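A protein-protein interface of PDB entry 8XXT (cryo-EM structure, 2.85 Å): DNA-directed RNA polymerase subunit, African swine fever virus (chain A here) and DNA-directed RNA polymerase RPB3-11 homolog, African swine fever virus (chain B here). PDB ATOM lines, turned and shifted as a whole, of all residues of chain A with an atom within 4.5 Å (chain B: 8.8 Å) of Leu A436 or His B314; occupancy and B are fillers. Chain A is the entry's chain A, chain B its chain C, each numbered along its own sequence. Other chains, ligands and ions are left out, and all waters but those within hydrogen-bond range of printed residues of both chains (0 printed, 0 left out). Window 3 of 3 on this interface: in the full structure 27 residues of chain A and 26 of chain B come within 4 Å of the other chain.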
ATOM      1  N   ASN A 330      10.191  14.128   7.062  1.00  0.00           N
ATOM      2  CA  ASN A 330       9.028  14.872   6.587  1.00  0.00           C
ATOM      3  C   ASN A 330       9.554  16.044   5.770  1.00  0.00           C
ATOM      4  O   ASN A 330       9.964  17.063   6.332  1.00  0.00           O
ATOM      5  CB  ASN A 330       8.160  15.341   7.744  1.00  0.00           C
ATOM      6  CG  ASN A 330       6.756  15.686   7.315  1.00  0.00           C
ATOM      7  OD1 ASN A 330       6.527  16.099   6.182  1.00  0.00           O
ATOM      8  ND2 ASN A 330       5.808  15.522   8.220  1.00  0.00           N
ATOM      9  N   ASP A 332       8.066  18.202   4.167  1.00  0.00           N
ATOM     10  CA  ASP A 332       7.200  19.371   4.194  1.00  0.00           C
ATOM     11  C   ASP A 332       7.335  20.172   5.479  1.00  0.00           C
ATOM     12  O   ASP A 332       6.537  21.085   5.713  1.00  0.00           O
ATOM     13  CB  ASP A 332       5.750  18.950   3.981  1.00  0.00           C
ATOM     14  CG  ASP A 332       5.455  18.622   2.536  1.00  0.00           C
ATOM     15  OD1 ASP A 332       6.015  19.292   1.645  1.00  0.00           O
ATOM     16  OD2 ASP A 332       4.673  17.683   2.287  1.00  0.00           O
ATOM     17  N   LEU A 333       8.316  19.853   6.313  1.00  0.00           N
ATOM     18  CA  LEU A 333       8.606  20.615   7.517  1.00  0.00           C
ATOM     19  C   LEU A 333       9.857  21.452   7.302  1.00  0.00           C
ATOM     20  O   LEU A 333      10.801  21.013   6.640  1.00  0.00           O
ATOM     21  CB  LEU A 333       8.802  19.694   8.720  1.00  0.00           C
ATOM     22  CG  LEU A 333       7.575  18.943   9.226  1.00  0.00           C
ATOM     23  CD1 LEU A 333       7.976  17.958  10.288  1.00  0.00           C
ATOM     24  CD2 LEU A 333       6.556  19.912   9.770  1.00  0.00           C
ATOM     25  N   GLY A 339       7.879  17.572  13.841  1.00  0.00           N
ATOM     26  CA  GLY A 339       6.531  17.046  13.842  1.00  0.00           C
ATOM     27  C   GLY A 339       6.202  16.326  15.132  1.00  0.00           C
ATOM     28  O   GLY A 339       6.769  15.271  15.423  1.00  0.00           O
ATOM     29  N   TYR A 340       5.284  16.885  15.912  1.00  0.00           N
ATOM     30  CA  TYR A 340       4.942  16.356  17.223  1.00  0.00           C
ATOM     31  C   TYR A 340       3.570  15.707  17.165  1.00  0.00           C
ATOM     32  O   TYR A 340       2.581  16.398  16.873  1.00  0.00           O
ATOM     33  CB  TYR A 340       4.962  17.466  18.268  1.00  0.00           C
ATOM     34  CG  TYR A 340       5.272  16.986  19.660  1.00  0.00           C
ATOM     35  CD1 TYR A 340       6.136  15.927  19.869  1.00  0.00           C
ATOM     36  CD2 TYR A 340       4.710  17.600  20.765  1.00  0.00           C
ATOM     37  CE1 TYR A 340       6.424  15.487  21.136  1.00  0.00           C
ATOM     38  CE2 TYR A 340       4.996  17.168  22.037  1.00  0.00           C
ATOM     39  CZ  TYR A 340       5.855  16.112  22.216  1.00  0.00           C
ATOM     40  OH  TYR A 340       6.145  15.673  23.485  1.00  0.00           O
ATOM     41  N   PRO A 341       3.450  14.406  17.419  1.00  0.00           N
ATOM     42  CA  PRO A 341       2.128  13.776  17.401  1.00  0.00           C
ATOM     43  C   PRO A 341       1.204  14.391  18.438  1.00  0.00           C
ATOM     44  O   PRO A 341       1.628  14.796  19.521  1.00  0.00           O
ATOM     45  CB  PRO A 341       2.430  12.307  17.714  1.00  0.00           C
ATOM     46  CG  PRO A 341       3.782  12.313  18.332  1.00  0.00           C
ATOM     47  CD  PRO A 341       4.518  13.433  17.686  1.00  0.00           C
ATOM     48  N   ILE A 342      -0.081  14.461  18.084  1.00  0.00           N
ATOM     49  CA  ILE A 342      -1.062  15.115  18.941  1.00  0.00           C
ATOM     50  C   ILE A 342      -1.221  14.375  20.263  1.00  0.00           C
ATOM     51  O   ILE A 342      -1.589  14.977  21.275  1.00  0.00           O
ATOM     52  CB  ILE A 342      -2.404  15.245  18.200  1.00  0.00           C
ATOM     53  CG1 ILE A 342      -3.373  16.117  18.990  1.00  0.00           C
ATOM     54  CG2 ILE A 342      -3.006  13.880  17.940  1.00  0.00           C
ATOM     55  CD1 ILE A 342      -4.585  16.529  18.203  1.00  0.00           C
ATOM     56  N   VAL A 434       5.299  21.440  15.303  1.00  0.00           N
ATOM     57  CA  VAL A 434       4.243  21.292  14.311  1.00  0.00           C
ATOM     58  C   VAL A 434       3.424  20.084  14.729  1.00  0.00           C
ATOM     59  O   VAL A 434       3.817  18.941  14.469  1.00  0.00           O
ATOM     60  CB  VAL A 434       4.798  21.120  12.892  1.00  0.00           C
ATOM     61  CG1 VAL A 434       3.669  20.908  11.910  1.00  0.00           C
ATOM     62  CG2 VAL A 434       5.612  22.327  12.500  1.00  0.00           C
ATOM     63  N   VAL A 435       2.294  20.324  15.383  1.00  0.00           N
ATOM     64  CA  VAL A 435       1.496  19.230  15.922  1.00  0.00           C
ATOM     65  C   VAL A 435       0.805  18.509  14.774  1.00  0.00           C
ATOM     66  O   VAL A 435       0.096  19.128  13.974  1.00  0.00           O
ATOM     67  CB  VAL A 435       0.480  19.735  16.952  1.00  0.00           C
ATOM     68  CG1 VAL A 435      -0.584  18.691  17.185  1.00  0.00           C
ATOM     69  CG2 VAL A 435       1.181  20.050  18.247  1.00  0.00           C
ATOM     70  N   LEU A 436       1.017  17.200  14.689  1.00  0.00           N
ATOM     71  CA  LEU A 436       0.393  16.365  13.673  1.00  0.00           C
ATOM     72  C   LEU A 436      -0.895  15.798  14.254  1.00  0.00           C
ATOM     73  O   LEU A 436      -0.861  15.001  15.195  1.00  0.00           O
ATOM     74  CB  LEU A 436       1.342  15.254  13.237  1.00  0.00           C
ATOM     75  CG  LEU A 436       2.794  15.683  13.035  1.00  0.00           C
ATOM     76  CD1 LEU A 436       3.667  14.475  12.822  1.00  0.00           C
ATOM     77  CD2 LEU A 436       2.919  16.639  11.869  1.00  0.00           C
ATOM     78  N   GLU A 437      -2.029  16.206  13.694  1.00  0.00           N
ATOM     79  CA  GLU A 437      -3.327  15.847  14.249  1.00  0.00           C
ATOM     80  C   GLU A 437      -3.797  14.463  13.828  1.00  0.00           C
ATOM     81  O   GLU A 437      -4.862  14.028  14.277  1.00  0.00           O
ATOM     82  CB  GLU A 437      -4.375  16.888  13.854  1.00  0.00           C
ATOM     83  CG  GLU A 437      -4.134  18.266  14.448  1.00  0.00           C
ATOM     84  CD  GLU A 437      -3.111  19.069  13.668  1.00  0.00           C
ATOM     85  OE1 GLU A 437      -2.730  18.635  12.561  1.00  0.00           O
ATOM     86  OE2 GLU A 437      -2.689  20.137  14.162  1.00  0.00           O
ATOM     87  N   ASN A 438      -3.048  13.768  12.986  1.00  0.00           N
ATOM     88  CA  ASN A 438      -3.414  12.409  12.617  1.00  0.00           C
ATOM     89  C   ASN A 438      -3.154  11.482  13.794  1.00  0.00           C
ATOM     90  O   ASN A 438      -2.006  11.376  14.244  1.00  0.00           O
ATOM     91  CB  ASN A 438      -2.619  11.961  11.396  1.00  0.00           C
ATOM     92  CG  ASN A 438      -3.189  10.715  10.753  1.00  0.00           C
ATOM     93  OD1 ASN A 438      -3.958   9.981  11.367  1.00  0.00           O
ATOM     94  ND2 ASN A 438      -2.814  10.472   9.505  1.00  0.00           N
ATOM     95  N   ILE A 441      -0.194   8.634  13.734  1.00  0.00           N
ATOM     96  CA  ILE A 441       1.221   8.976  13.676  1.00  0.00           C
ATOM     97  C   ILE A 441       1.743   9.103  15.099  1.00  0.00           C
ATOM     98  O   ILE A 441       1.136   9.788  15.932  1.00  0.00           O
ATOM     99  CB  ILE A 441       1.452  10.275  12.884  1.00  0.00           C
ATOM    100  CG1 ILE A 441       1.679   9.978  11.400  1.00  0.00           C
ATOM    101  CG2 ILE A 441       2.645  11.031  13.430  1.00  0.00           C
ATOM    102  CD1 ILE A 441       0.524   9.305  10.710  1.00  0.00           C
ATOM    103  N   GLN A 445       8.726  13.843  13.495  1.00  0.00           N
ATOM    104  CA  GLN A 445       8.997  14.105  12.092  1.00  0.00           C
ATOM    105  C   GLN A 445       9.835  15.365  11.971  1.00  0.00           C
ATOM    106  O   GLN A 445       9.511  16.393  12.572  1.00  0.00           O
ATOM    107  CB  GLN A 445       7.695  14.235  11.308  1.00  0.00           C
ATOM    108  CG  GLN A 445       6.729  13.108  11.597  1.00  0.00           C
ATOM    109  CD  GLN A 445       5.881  12.742  10.410  1.00  0.00           C
ATOM    110  OE1 GLN A 445       5.470  13.602   9.637  1.00  0.00           O
ATOM    111  NE2 GLN A 445       5.616  11.454  10.252  1.00  0.00           N
ATOM    112  N   LYS B 283     -10.393  21.332   4.105  1.00  0.00           N
ATOM    113  CA  LYS B 283      -9.937  20.195   4.884  1.00  0.00           C
ATOM    114  C   LYS B 283     -10.423  18.893   4.265  1.00  0.00           C
ATOM    115  O   LYS B 283     -11.496  18.833   3.661  1.00  0.00           O
ATOM    116  CB  LYS B 283     -10.434  20.301   6.326  1.00  0.00           C
ATOM    117  CG  LYS B 283      -9.708  21.338   7.158  1.00  0.00           C
ATOM    118  CD  LYS B 283      -8.295  20.895   7.479  1.00  0.00           C
ATOM    119  CE  LYS B 283      -8.283  19.551   8.189  1.00  0.00           C
ATOM    120  NZ  LYS B 283      -7.020  19.343   8.949  1.00  0.00           N
ATOM    121  N   GLN B 310      -1.386  22.671  -2.860  1.00  0.00           N
ATOM    122  CA  GLN B 310      -0.572  21.711  -2.136  1.00  0.00           C
ATOM    123  C   GLN B 310      -1.432  20.973  -1.126  1.00  0.00           C
ATOM    124  O   GLN B 310      -2.102  21.598  -0.300  1.00  0.00           O
ATOM    125  CB  GLN B 310       0.612  22.391  -1.442  1.00  0.00           C
ATOM    126  CG  GLN B 310       0.248  23.580  -0.587  1.00  0.00           C
ATOM    127  CD  GLN B 310       1.394  24.021   0.288  1.00  0.00           C
ATOM    128  OE1 GLN B 310       2.327  23.259   0.536  1.00  0.00           O
ATOM    129  NE2 GLN B 310       1.336  25.261   0.761  1.00  0.00           N
ATOM    130  N   CYS B 311      -1.424  19.648  -1.210  1.00  0.00           N
ATOM    131  CA  CYS B 311      -2.047  18.787  -0.213  1.00  0.00           C
ATOM    132  C   CYS B 311      -0.913  18.164   0.589  1.00  0.00           C
ATOM    133  O   CYS B 311      -0.449  17.062   0.299  1.00  0.00           O
ATOM    134  CB  CYS B 311      -2.926  17.729  -0.858  1.00  0.00           C
ATOM    135  SG  CYS B 311      -4.310  18.372  -1.803  1.00  0.00           S
ATOM    136  N   VAL B 312      -0.457  18.892   1.602  1.00  0.00           N
ATOM    137  CA  VAL B 312       0.585  18.353   2.478  1.00  0.00           C
ATOM    138  C   VAL B 312       0.040  17.119   3.183  1.00  0.00           C
ATOM    139  O   VAL B 312      -1.118  17.135   3.644  1.00  0.00           O
ATOM    140  CB  VAL B 312       1.038  19.417   3.491  1.00  0.00           C
ATOM    141  CG1 VAL B 312       2.129  18.876   4.377  1.00  0.00           C
ATOM    142  CG2 VAL B 312       1.516  20.656   2.769  1.00  0.00           C
ATOM    143  N   PRO B 313       0.794  16.020   3.259  1.00  0.00           N
ATOM    144  CA  PRO B 313       0.253  14.812   3.901  1.00  0.00           C
ATOM    145  C   PRO B 313      -0.237  15.047   5.317  1.00  0.00           C
ATOM    146  O   PRO B 313      -1.272  14.489   5.705  1.00  0.00           O
ATOM    147  CB  PRO B 313       1.439  13.845   3.853  1.00  0.00           C
ATOM    148  CG  PRO B 313       2.192  14.267   2.643  1.00  0.00           C
ATOM    149  CD  PRO B 313       2.074  15.758   2.584  1.00  0.00           C
ATOM    150  N   HIS B 314       0.460  15.860   6.099  1.00  0.00           N
ATOM    151  CA  HIS B 314      -0.103  16.296   7.365  1.00  0.00           C
ATOM    152  C   HIS B 314      -0.867  17.600   7.162  1.00  0.00           C
ATOM    153  O   HIS B 314      -0.751  18.260   6.129  1.00  0.00           O
ATOM    154  CB  HIS B 314       0.980  16.446   8.437  1.00  0.00           C
ATOM    155  CG  HIS B 314       2.007  17.491   8.135  1.00  0.00           C
ATOM    156  ND1 HIS B 314       3.088  17.257   7.316  1.00  0.00           N
ATOM    157  CD2 HIS B 314       2.133  18.766   8.570  1.00  0.00           C
ATOM    158  CE1 HIS B 314       3.829  18.348   7.246  1.00  0.00           C
ATOM    159  NE2 HIS B 314       3.270  19.280   7.995  1.00  0.00           N
ATOM    160  N   LYS B 315      -1.682  17.939   8.163  1.00  0.00           N
ATOM    161  CA  LYS B 315      -2.659  19.026   8.128  1.00  0.00           C
ATOM    162  C   LYS B 315      -3.861  18.648   7.269  1.00  0.00           C
ATOM    163  O   LYS B 315      -4.870  19.359   7.271  1.00  0.00           O
ATOM    164  CB  LYS B 315      -2.040  20.338   7.634  1.00  0.00           C
ATOM    165  CG  LYS B 315      -0.831  20.793   8.430  1.00  0.00           C
ATOM    166  CD  LYS B 315      -0.507  22.248   8.155  1.00  0.00           C
ATOM    167  CE  LYS B 315      -0.007  22.438   6.737  1.00  0.00           C
ATOM    168  NZ  LYS B 315      -0.532  23.688   6.125  1.00  0.00           N
ATOM    169  N   GLN B 316      -3.760  17.527   6.560  1.00  0.00           N
ATOM    170  CA  GLN B 316      -4.878  16.847   5.902  1.00  0.00           C
ATOM    171  C   GLN B 316      -5.850  17.825   5.245  1.00  0.00           C
ATOM    172  O   GLN B 316      -7.044  17.856   5.537  1.00  0.00           O
ATOM    173  CB  GLN B 316      -5.602  15.946   6.898  1.00  0.00           C
ATOM    174  CG  GLN B 316      -4.661  15.049   7.684  1.00  0.00           C
ATOM    175  CD  GLN B 316      -5.358  14.279   8.780  1.00  0.00           C
ATOM    176  OE1 GLN B 316      -5.792  14.852   9.778  1.00  0.00           O
ATOM    177  NE2 GLN B 316      -5.462  12.968   8.607  1.00  0.00           N
ATOM    178  N   GLU B 317      -5.313  18.633   4.333  1.00  0.00           N
ATOM    179  CA  GLU B 317      -6.106  19.672   3.698  1.00  0.00           C
ATOM    180  C   GLU B 317      -5.540  19.987   2.323  1.00  0.00           C
ATOM    181  O   GLU B 317      -4.385  19.682   2.021  1.00  0.00           O
ATOM    182  CB  GLU B 317      -6.137  20.944   4.546  1.00  0.00           C
ATOM    183  CG  GLU B 317      -4.815  21.675   4.572  1.00  0.00           C
ATOM    184  CD  GLU B 317      -4.800  22.813   5.562  1.00  0.00           C
ATOM    185  OE1 GLU B 317      -5.813  22.994   6.268  1.00  0.00           O
ATOM    186  OE2 GLU B 317      -3.776  23.522   5.638  1.00  0.00           O
ATOM    187  N   MET B 318      -6.373  20.611   1.496  1.00  0.00           N
ATOM    188  CA  MET B 318      -5.970  21.140   0.200  1.00  0.00           C
ATOM    189  C   MET B 318      -5.939  22.657   0.293  1.00  0.00           C
ATOM    190  O   MET B 318      -6.950  23.280   0.630  1.00  0.00           O
ATOM    191  CB  MET B 318      -6.929  20.694  -0.901  1.00  0.00           C
ATOM    192  CG  MET B 318      -6.485  21.070  -2.304  1.00  0.00           C
ATOM    193  SD  MET B 318      -7.258  22.576  -2.917  1.00  0.00           S
ATOM    194  CE  MET B 318      -8.891  22.436  -2.204  1.00  0.00           C
ATOM    195  N   VAL B 319      -4.785  23.246  -0.003  1.00  0.00           N
ATOM    196  CA  VAL B 319      -4.608  24.692   0.019  1.00  0.00           C
ATOM    197  C   VAL B 319      -4.283  25.138  -1.396  1.00  0.00           C
ATOM    198  O   VAL B 319      -3.239  24.764  -1.942  1.00  0.00           O
ATOM    199  CB  VAL B 319      -3.504  25.119   0.995  1.00  0.00           C
ATOM    200  CG1 VAL B 319      -3.161  26.581   0.799  1.00  0.00           C
ATOM    201  CG2 VAL B 319      -3.935  24.861   2.420  1.00  0.00           C
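Printed residues of chain A that touch a printed residue of chain B: Asn A330, Asp A332, Leu A333, Leu A436 and Asn A438.
Hydrophobic or aromatic side chains of chain A within 4 Å of the printed part of chain B: Leu A333 and Leu A436.
Printed residues of chain B that touch a printed residue of chain A: Val B312, Pro B313, His B314 and Gln B316.
Hydrophobic or aromatic side chains of chain B within 4 Å of the printed part of chain A: Val B312, Pro B313 and His B314.
Val B312 touches Asp A332.
OD2 of Asp A332 touches CD of Pro B313, at 3.2 Å.
Asp A332 touches His B314.
Leu A333 touches His B314 (CD2 to NE2, 3.8 Å).
Leu A436 touches His B314.
NE2 of Gln B316 touches ND2 of Asn A438, 3.7 Å away.
ND2 of Asn A330 sits at hydrogen-bond distance from ND1 of His B314 (3.4 Å).
The backbone carbonyl oxygen (O) of Tyr A340 is in hydrogen-bond range of the backbone NH (N) of Leu A436 (2.8 Å).
The side-chain amide oxygen (OD1) of Asn A330 lies close to the backbone NH (N) of Asp A332, at 3.3 Å.
OE1 of Gln A445 sits at hydrogen-bond distance from ND2 of Asn A330, at 2.4 Å.
The backbone NH (N) of Ile A342 lies within hydrogen-bond range of the backbone carbonyl oxygen (O) of Leu A436 (3.0 Å).
Printed residues of chain B within 4 Å of Asp A332: Val B312 (3.5 Å), Pro B313 (3.2 Å) and His B314 (3.8 Å).
Val A435 touches none of the printed residues of chain B.
Leu A436 touches just one residue of chain B: His B314.
No residue of chain B comes within 4 Å of Glu A437.
Of the printed residues of chain B, Asn A438 touches Gln B316.
Gln B310 touches none of the printed residues of chain A.
Of the printed residues of chain A, Val B312 touches Asp A332.
Of the printed residues of chain A, Pro B313 touches Asp A332.
His B314 touches four residues of chain A.
Printed residues of chain A within 4 Å of Gln B316: Asn A438.
The nearest residue of chain A that does not touch His B314 is Val A434 (4.3 Å).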
